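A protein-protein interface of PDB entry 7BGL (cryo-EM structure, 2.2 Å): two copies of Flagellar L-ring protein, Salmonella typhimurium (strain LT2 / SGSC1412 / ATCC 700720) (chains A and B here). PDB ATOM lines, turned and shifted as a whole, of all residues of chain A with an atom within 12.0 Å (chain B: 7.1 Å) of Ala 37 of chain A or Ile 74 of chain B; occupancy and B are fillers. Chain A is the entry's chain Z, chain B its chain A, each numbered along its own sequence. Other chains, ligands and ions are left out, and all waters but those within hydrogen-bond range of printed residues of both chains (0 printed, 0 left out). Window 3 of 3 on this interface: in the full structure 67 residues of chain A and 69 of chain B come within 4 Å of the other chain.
The backbone carbonyl oxygen of Val 164 of chain B lies close to the backbone carbonyl oxygen of Thr 35 of chain A (3.5 Å).
The backbone carbonyl oxygen (O) of Ile 74 of chain B sits close to the backbone carbonyl oxygen (O) of Val 152 of chain B (2.4 Å).
N of Val 164 of chain B is in hydrogen-bond range of O of Thr 151 of chain B (2.9 Å).
The backbone carbonyl oxygen (O) of Asp 76 of chain B sits at hydrogen-bond distance from the backbone NH (N) of Val 152 of chain B.
Among the printed residues, pairs that only touch across the chains: Ala 34 of chain A with Val 164 of chain B, Ala 37 of chain A with Ile 74 of chain B, Ala 37 of chain A with Gly 75 of chain B, Ala 37 of chain A with Val 152 of chain B, Gln 38 of chain A with Ile 74 of chain B, Pro 39 of chain A with Gly 75 of chain B and Ile 40 of chain A with Ile 74 of chain B.
Of the printed residues of chain B, Ala 34 of chain A touches Val 164 (3.6 Å).
Printed residues of chain B within 4 Å of Gln 38 of chain A: Ile 74 (3.97 Å).
Printed residues of chain B within 4 Å of Pro 39 of chain A: Gly 75 (3.6 Å).
Of the printed residues of chain B, Ile 40 of chain A touches Ile 74.
No residue of chain A comes within 4 Å of Asn 73 of chain B.
Printed residues of chain A within 4 Å of Ile 74 of chain B: Ala 37, Gln 38 and Ile 40.
Of the printed residues of chain A, Gly 75 of chain B touches Ala 37 (3.98 Å) and Pro 39 (3.6 Å).
No residue of chain A comes within 4 Å of Thr 151 of chain B.
Asp 153 of chain B touches none of the printed residues of chain A.
No residue of chain A comes within 4 Å of Gln 154 of chain B.
No residue of chain A comes within 4 Å of Val 155 of chain B.
Of chain A, only Ala 34 (3.6 Å) and Thr 35 (3.5 Å) come within 4 Å of Val 164 of chain B.
Printed residues of chain A that touch a printed residue of chain B: Ala 34, Thr 35, Ala 37, Gln 38, Pro 39 and Ile 40.
Of the 14 printed residues of chain B, 4 touch a printed residue of chain A.
Printed residues of chain B that touch a printed residue of chain A: Ile 74, Gly 75, Val 152 and Val 164.
Among the printed residues, no Asp or Glu carboxylate lies within 4 Å of a Lys or Arg side-chain nitrogen of the other chain.
No position is printed for both chains.
Of the 8 pairs that touch across the chains among the printed residues, none has its exchanged pair printed and touching as well.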
ATOM      1  N   VAL A  31     -21.611  -1.548  21.125  1.00  0.00           N
ATOM      2  CA  VAL A  31     -20.233  -1.566  20.607  1.00  0.00           C
ATOM      3  C   VAL A  31     -19.892  -3.033  20.378  1.00  0.00           C
ATOM      4  O   VAL A  31     -19.285  -3.713  21.207  1.00  0.00           O
ATOM      5  CB  VAL A  31     -19.250  -0.866  21.550  1.00  0.00           C
ATOM      6  CG1 VAL A  31     -17.838  -0.948  20.994  1.00  0.00           C
ATOM      7  CG2 VAL A  31     -19.660   0.582  21.761  1.00  0.00           C
ATOM      8  N   GLN A  32     -20.297  -3.534  19.217  1.00  0.00           N
ATOM      9  CA  GLN A  32     -20.080  -4.926  18.860  1.00  0.00           C
ATOM     10  C   GLN A  32     -18.700  -5.116  18.242  1.00  0.00           C
ATOM     11  O   GLN A  32     -18.043  -4.164  17.815  1.00  0.00           O
ATOM     12  CB  GLN A  32     -21.158  -5.410  17.890  1.00  0.00           C
ATOM     13  CG  GLN A  32     -22.572  -5.299  18.432  1.00  0.00           C
ATOM     14  CD  GLN A  32     -23.608  -5.842  17.469  1.00  0.00           C
ATOM     15  OE1 GLN A  32     -23.269  -6.439  16.447  1.00  0.00           O
ATOM     16  NE2 GLN A  32     -24.879  -5.638  17.790  1.00  0.00           N
ATOM     17  N   GLY A  33     -18.267  -6.372  18.198  1.00  0.00           N
ATOM     18  CA  GLY A  33     -16.971  -6.705  17.647  1.00  0.00           C
ATOM     19  C   GLY A  33     -15.860  -6.584  18.667  1.00  0.00           C
ATOM     20  O   GLY A  33     -16.044  -6.153  19.808  1.00  0.00           O
ATOM     21  N   ALA A  34     -14.667  -6.981  18.235  1.00  0.00           N
ATOM     22  CA  ALA A  34     -13.503  -6.922  19.104  1.00  0.00           C
ATOM     23  C   ALA A  34     -13.170  -5.478  19.453  1.00  0.00           C
ATOM     24  O   ALA A  34     -13.265  -4.579  18.614  1.00  0.00           O
ATOM     25  CB  ALA A  34     -12.304  -7.591  18.435  1.00  0.00           C
ATOM     26  N   THR A  35     -12.777  -5.258  20.705  1.00  0.00           N
ATOM     27  CA  THR A  35     -12.335  -3.953  21.173  1.00  0.00           C
ATOM     28  C   THR A  35     -10.822  -3.807  21.126  1.00  0.00           C
ATOM     29  O   THR A  35     -10.279  -2.872  21.720  1.00  0.00           O
ATOM     30  CB  THR A  35     -12.837  -3.697  22.595  1.00  0.00           C
ATOM     31  OG1 THR A  35     -12.245  -4.647  23.490  1.00  0.00           O
ATOM     32  CG2 THR A  35     -14.351  -3.817  22.658  1.00  0.00           C
ATOM     33  N   THR A  36     -10.132  -4.718  20.444  1.00  0.00           N
ATOM     34  CA  THR A  36      -8.679  -4.731  20.386  1.00  0.00           C
ATOM     35  C   THR A  36      -8.213  -4.935  18.955  1.00  0.00           C
ATOM     36  O   THR A  36      -8.877  -5.612  18.164  1.00  0.00           O
ATOM     37  CB  THR A  36      -8.102  -5.837  21.268  1.00  0.00           C
ATOM     38  OG1 THR A  36      -9.105  -6.833  21.500  1.00  0.00           O
ATOM     39  CG2 THR A  36      -7.660  -5.269  22.587  1.00  0.00           C
ATOM     40  N   ALA A  37      -7.065  -4.348  18.631  1.00  0.00           N
ATOM     41  CA  ALA A  37      -6.416  -4.537  17.342  1.00  0.00           C
ATOM     42  C   ALA A  37      -4.956  -4.882  17.587  1.00  0.00           C
ATOM     43  O   ALA A  37      -4.248  -4.140  18.275  1.00  0.00           O
ATOM     44  CB  ALA A  37      -6.541  -3.286  16.471  1.00  0.00           C
ATOM     45  N   GLN A  38      -4.516  -6.005  17.041  1.00  0.00           N
ATOM     46  CA  GLN A  38      -3.114  -6.381  17.155  1.00  0.00           C
ATOM     47  C   GLN A  38      -2.292  -5.598  16.137  1.00  0.00           C
ATOM     48  O   GLN A  38      -2.580  -5.659  14.937  1.00  0.00           O
ATOM     49  CB  GLN A  38      -2.941  -7.881  16.935  1.00  0.00           C
ATOM     50  CG  GLN A  38      -3.351  -8.738  18.120  1.00  0.00           C
ATOM     51  CD  GLN A  38      -3.018  -8.090  19.449  1.00  0.00           C
ATOM     52  OE1 GLN A  38      -1.851  -7.882  19.777  1.00  0.00           O
ATOM     53  NE2 GLN A  38      -4.047  -7.771  20.225  1.00  0.00           N
ATOM     54  N   PRO A  39      -1.275  -4.855  16.566  1.00  0.00           N
ATOM     55  CA  PRO A  39      -0.470  -4.091  15.606  1.00  0.00           C
ATOM     56  C   PRO A  39       0.240  -5.002  14.617  1.00  0.00           C
ATOM     57  O   PRO A  39       0.649  -6.118  14.945  1.00  0.00           O
ATOM     58  CB  PRO A  39       0.528  -3.342  16.497  1.00  0.00           C
ATOM     59  CG  PRO A  39       0.582  -4.134  17.760  1.00  0.00           C
ATOM     60  CD  PRO A  39      -0.793  -4.694  17.947  1.00  0.00           C
ATOM     61  N   ILE A  40       0.382  -4.509  13.391  1.00  0.00           N
ATOM     62  CA  ILE A  40       1.074  -5.230  12.325  1.00  0.00           C
ATOM     63  C   ILE A  40       2.571  -4.971  12.436  1.00  0.00           C
ATOM     64  O   ILE A  40       2.984  -3.822  12.647  1.00  0.00           O
ATOM     65  CB  ILE A  40       0.548  -4.820  10.941  1.00  0.00           C
ATOM     66  CG1 ILE A  40       0.149  -3.343  10.941  1.00  0.00           C
ATOM     67  CG2 ILE A  40      -0.627  -5.690  10.532  1.00  0.00           C
ATOM     68  CD1 ILE A  40      -0.913  -2.999   9.923  1.00  0.00           C
ATOM     69  N   PRO A  41       3.418  -5.995  12.307  1.00  0.00           N
ATOM     70  CA  PRO A  41       4.868  -5.742  12.358  1.00  0.00           C
ATOM     71  C   PRO A  41       5.341  -4.780  11.284  1.00  0.00           C
ATOM     72  O   PRO A  41       6.282  -4.010  11.514  1.00  0.00           O
ATOM     73  CB  PRO A  41       5.474  -7.141  12.177  1.00  0.00           C
ATOM     74  CG  PRO A  41       4.390  -8.086  12.578  1.00  0.00           C
ATOM     75  CD  PRO A  41       3.108  -7.427  12.175  1.00  0.00           C
ATOM     76  N   GLY A  42       4.713  -4.801  10.112  1.00  0.00           N
ATOM     77  CA  GLY A  42       5.096  -3.935   9.025  1.00  0.00           C
ATOM     78  C   GLY A  42       5.869  -4.674   7.953  1.00  0.00           C
ATOM     79  O   GLY A  42       5.987  -5.904   7.973  1.00  0.00           O
ATOM     80  N   PRO A  43       6.416  -3.933   6.989  1.00  0.00           N
ATOM     81  CA  PRO A  43       7.174  -4.563   5.905  1.00  0.00           C
ATOM     82  C   PRO A  43       8.653  -4.682   6.231  1.00  0.00           C
ATOM     83  O   PRO A  43       9.264  -3.793   6.828  1.00  0.00           O
ATOM     84  CB  PRO A  43       6.944  -3.605   4.728  1.00  0.00           C
ATOM     85  CG  PRO A  43       6.611  -2.263   5.366  1.00  0.00           C
ATOM     86  CD  PRO A  43       6.366  -2.469   6.842  1.00  0.00           C
ATOM     87  N   ALA A  55       6.161   3.022   3.948  1.00  0.00           N
ATOM     88  CA  ALA A  55       5.126   2.277   4.655  1.00  0.00           C
ATOM     89  C   ALA A  55       3.880   2.126   3.791  1.00  0.00           C
ATOM     90  O   ALA A  55       2.751   2.203   4.284  1.00  0.00           O
ATOM     91  CB  ALA A  55       4.778   2.944   5.985  1.00  0.00           C
ATOM     92  N   GLN A  56       4.067   1.902   2.490  1.00  0.00           N
ATOM     93  CA  GLN A  56       2.940   1.628   1.606  1.00  0.00           C
ATOM     94  C   GLN A  56       1.930   2.770   1.637  1.00  0.00           C
ATOM     95  O   GLN A  56       0.850   2.626   2.223  1.00  0.00           O
ATOM     96  CB  GLN A  56       2.264   0.313   1.996  1.00  0.00           C
ATOM     97  CG  GLN A  56       3.209  -0.878   2.046  1.00  0.00           C
ATOM     98  CD  GLN A  56       2.846  -1.865   3.137  1.00  0.00           C
ATOM     99  OE1 GLN A  56       2.131  -1.530   4.081  1.00  0.00           O
ATOM    100  NE2 GLN A  56       3.338  -3.093   3.013  1.00  0.00           N
ATOM    101  N   ILE A  58      -1.088   5.235   1.194  1.00  0.00           N
ATOM    102  CA  ILE A  58      -2.464   4.856   0.900  1.00  0.00           C
ATOM    103  C   ILE A  58      -3.092   5.818  -0.100  1.00  0.00           C
ATOM    104  O   ILE A  58      -3.485   5.416  -1.200  1.00  0.00           O
ATOM    105  CB  ILE A  58      -3.303   4.787   2.190  1.00  0.00           C
ATOM    106  CG1 ILE A  58      -3.052   6.022   3.058  1.00  0.00           C
ATOM    107  CG2 ILE A  58      -2.983   3.517   2.964  1.00  0.00           C
ATOM    108  CD1 ILE A  58      -3.953   6.110   4.271  1.00  0.00           C
ATOM    109  N   ARG B  72      -1.337   6.084  13.744  1.00  0.00           N
ATOM    110  CA  ARG B  72      -1.218   5.919  12.301  1.00  0.00           C
ATOM    111  C   ARG B  72      -1.474   4.507  11.803  1.00  0.00           C
ATOM    112  O   ARG B  72      -1.804   4.349  10.621  1.00  0.00           O
ATOM    113  CB  ARG B  72       0.175   6.359  11.827  1.00  0.00           C
ATOM    114  CG  ARG B  72       0.369   7.865  11.808  1.00  0.00           C
ATOM    115  CD  ARG B  72       1.642   8.252  11.077  1.00  0.00           C
ATOM    116  NE  ARG B  72       2.122   9.566  11.485  1.00  0.00           N
ATOM    117  CZ  ARG B  72       2.763   9.810  12.620  1.00  0.00           C
ATOM    118  NH1 ARG B  72       3.023   8.846  13.487  1.00  0.00           N
ATOM    119  NH2 ARG B  72       3.153  11.051  12.891  1.00  0.00           N
ATOM    120  N   ASN B  73      -1.342   3.486  12.639  1.00  0.00           N
ATOM    121  CA  ASN B  73      -1.489   2.102  12.213  1.00  0.00           C
ATOM    122  C   ASN B  73      -2.584   1.421  13.033  1.00  0.00           C
ATOM    123  O   ASN B  73      -3.252   2.044  13.860  1.00  0.00           O
ATOM    124  CB  ASN B  73      -0.153   1.367  12.327  1.00  0.00           C
ATOM    125  CG  ASN B  73       0.907   1.942  11.409  1.00  0.00           C
ATOM    126  OD1 ASN B  73       1.519   2.964  11.713  1.00  0.00           O
ATOM    127  ND2 ASN B  73       1.128   1.286  10.276  1.00  0.00           N
ATOM    128  N   ILE B  74      -2.756   0.120  12.794  1.00  0.00           N
ATOM    129  CA  ILE B  74      -3.836  -0.622  13.439  1.00  0.00           C
ATOM    130  C   ILE B  74      -3.641  -0.648  14.951  1.00  0.00           C
ATOM    131  O   ILE B  74      -4.583  -0.427  15.719  1.00  0.00           O
ATOM    132  CB  ILE B  74      -3.929  -2.043  12.858  1.00  0.00           C
ATOM    133  CG1 ILE B  74      -4.202  -1.985  11.354  1.00  0.00           C
ATOM    134  CG2 ILE B  74      -5.013  -2.837  13.566  1.00  0.00           C
ATOM    135  CD1 ILE B  74      -5.641  -1.692  11.007  1.00  0.00           C
ATOM    136  N   GLY B  75      -2.421  -0.915  15.400  1.00  0.00           N
ATOM    137  CA  GLY B  75      -2.187  -1.057  16.821  1.00  0.00           C
ATOM    138  C   GLY B  75      -2.053   0.224  17.609  1.00  0.00           C
ATOM    139  O   GLY B  75      -1.952   0.171  18.837  1.00  0.00           O
ATOM    140  N   ASP B  76      -2.053   1.378  16.949  1.00  0.00           N
ATOM    141  CA  ASP B  76      -1.853   2.639  17.646  1.00  0.00           C
ATOM    142  C   ASP B  76      -3.015   2.930  18.589  1.00  0.00           C
ATOM    143  O   ASP B  76      -4.167   2.578  18.324  1.00  0.00           O
ATOM    144  CB  ASP B  76      -1.689   3.780  16.645  1.00  0.00           C
ATOM    145  CG  ASP B  76      -0.359   3.731  15.920  1.00  0.00           C
ATOM    146  OD1 ASP B  76       0.416   2.782  16.163  1.00  0.00           O
ATOM    147  OD2 ASP B  76      -0.087   4.640  15.107  1.00  0.00           O
ATOM    148  N   THR B  77      -2.698   3.584  19.703  1.00  0.00           N
ATOM    149  CA  THR B  77      -3.671   3.908  20.733  1.00  0.00           C
ATOM    150  C   THR B  77      -3.918   5.410  20.776  1.00  0.00           C
ATOM    151  O   THR B  77      -3.008   6.214  20.555  1.00  0.00           O
ATOM    152  CB  THR B  77      -3.204   3.425  22.109  1.00  0.00           C
ATOM    153  OG1 THR B  77      -1.914   3.975  22.399  1.00  0.00           O
ATOM    154  CG2 THR B  77      -3.119   1.908  22.140  1.00  0.00           C
ATOM    155  N   THR B 151      -8.076   2.024  20.848  1.00  0.00           N
ATOM    156  CA  THR B 151      -7.102   1.504  19.901  1.00  0.00           C
ATOM    157  C   THR B 151      -7.671   1.580  18.492  1.00  0.00           C
ATOM    158  O   THR B 151      -8.875   1.394  18.287  1.00  0.00           O
ATOM    159  CB  THR B 151      -6.722   0.057  20.229  1.00  0.00           C
ATOM    160  OG1 THR B 151      -6.315  -0.035  21.600  1.00  0.00           O
ATOM    161  CG2 THR B 151      -5.583  -0.409  19.338  1.00  0.00           C
ATOM    162  N   VAL B 152      -6.799   1.853  17.521  1.00  0.00           N
ATOM    163  CA  VAL B 152      -7.238   1.924  16.134  1.00  0.00           C
ATOM    164  C   VAL B 152      -7.673   0.544  15.663  1.00  0.00           C
ATOM    165  O   VAL B 152      -7.019  -0.468  15.943  1.00  0.00           O
ATOM    166  CB  VAL B 152      -6.118   2.488  15.243  1.00  0.00           C
ATOM    167  CG1 VAL B 152      -6.502   2.379  13.778  1.00  0.00           C
ATOM    168  CG2 VAL B 152      -5.820   3.930  15.616  1.00  0.00           C
ATOM    169  N   ASP B 153      -8.796   0.495  14.952  1.00  0.00           N
ATOM    170  CA  ASP B 153      -9.299  -0.747  14.381  1.00  0.00           C
ATOM    171  C   ASP B 153      -8.891  -0.933  12.928  1.00  0.00           C
ATOM    172  O   ASP B 153      -8.559  -2.049  12.519  1.00  0.00           O
ATOM    173  CB  ASP B 153     -10.826  -0.800  14.491  1.00  0.00           C
ATOM    174  CG  ASP B 153     -11.369  -2.206  14.353  1.00  0.00           C
ATOM    175  OD1 ASP B 153     -11.910  -2.532  13.275  1.00  0.00           O
ATOM    176  OD2 ASP B 153     -11.255  -2.987  15.320  1.00  0.00           O
ATOM    177  N   GLN B 154      -8.911   0.138  12.140  1.00  0.00           N
ATOM    178  CA  GLN B 154      -8.488   0.083  10.750  1.00  0.00           C
ATOM    179  C   GLN B 154      -8.308   1.505  10.245  1.00  0.00           C
ATOM    180  O   GLN B 154      -8.802   2.463  10.845  1.00  0.00           O
ATOM    181  CB  GLN B 154      -9.495  -0.677   9.882  1.00  0.00           C
ATOM    182  CG  GLN B 154     -10.925  -0.194  10.030  1.00  0.00           C
ATOM    183  CD  GLN B 154     -11.820  -0.688   8.913  1.00  0.00           C
ATOM    184  OE1 GLN B 154     -11.343  -1.189   7.895  1.00  0.00           O
ATOM    185  NE2 GLN B 154     -13.127  -0.549   9.096  1.00  0.00           N
ATOM    186  N   VAL B 155      -7.593   1.629   9.133  1.00  0.00           N
ATOM    187  CA  VAL B 155      -7.334   2.914   8.495  1.00  0.00           C
ATOM    188  C   VAL B 155      -8.196   2.994   7.243  1.00  0.00           C
ATOM    189  O   VAL B 155      -8.131   2.112   6.379  1.00  0.00           O
ATOM    190  CB  VAL B 155      -5.848   3.094   8.159  1.00  0.00           C
ATOM    191  CG1 VAL B 155      -5.597   4.484   7.599  1.00  0.00           C
ATOM    192  CG2 VAL B 155      -4.995   2.852   9.392  1.00  0.00           C
ATOM    193  N   LEU B 161      -9.342   7.136  11.039  1.00  0.00           N
ATOM    194  CA  LEU B 161      -9.055   5.962  11.850  1.00  0.00           C
ATOM    195  C   LEU B 161     -10.325   5.493  12.541  1.00  0.00           C
ATOM    196  O   LEU B 161     -11.035   6.296  13.157  1.00  0.00           O
ATOM    197  CB  LEU B 161      -7.975   6.268  12.889  1.00  0.00           C
ATOM    198  CG  LEU B 161      -6.768   7.068  12.402  1.00  0.00           C
ATOM    199  CD1 LEU B 161      -6.048   7.713  13.573  1.00  0.00           C
ATOM    200  CD2 LEU B 161      -5.825   6.178  11.612  1.00  0.00           C
ATOM    201  N   HIS B 162     -10.610   4.199  12.434  1.00  0.00           N
ATOM    202  CA  HIS B 162     -11.706   3.581  13.171  1.00  0.00           C
ATOM    203  C   HIS B 162     -11.162   3.113  14.515  1.00  0.00           C
ATOM    204  O   HIS B 162     -10.337   2.196  14.575  1.00  0.00           O
ATOM    205  CB  HIS B 162     -12.311   2.423  12.384  1.00  0.00           C
ATOM    206  CG  HIS B 162     -13.532   1.839  13.023  1.00  0.00           C
ATOM    207  ND1 HIS B 162     -13.518   0.633  13.690  1.00  0.00           N
ATOM    208  CD2 HIS B 162     -14.803   2.297  13.100  1.00  0.00           C
ATOM    209  CE1 HIS B 162     -14.728   0.373  14.150  1.00  0.00           C
ATOM    210  NE2 HIS B 162     -15.527   1.367  13.805  1.00  0.00           N
ATOM    211  N   VAL B 164     -11.714   1.702  18.425  1.00  0.00           N
ATOM    212  CA  VAL B 164     -12.546   0.927  19.336  1.00  0.00           C
ATOM    213  C   VAL B 164     -11.759   0.705  20.618  1.00  0.00           C
ATOM    214  O   VAL B 164     -10.569   0.371  20.571  1.00  0.00           O
ATOM    215  CB  VAL B 164     -12.974  -0.418  18.719  1.00  0.00           C
ATOM    216  CG1 VAL B 164     -11.773  -1.332  18.560  1.00  0.00           C
ATOM    217  CG2 VAL B 164     -14.037  -1.077  19.579  1.00  0.00           C
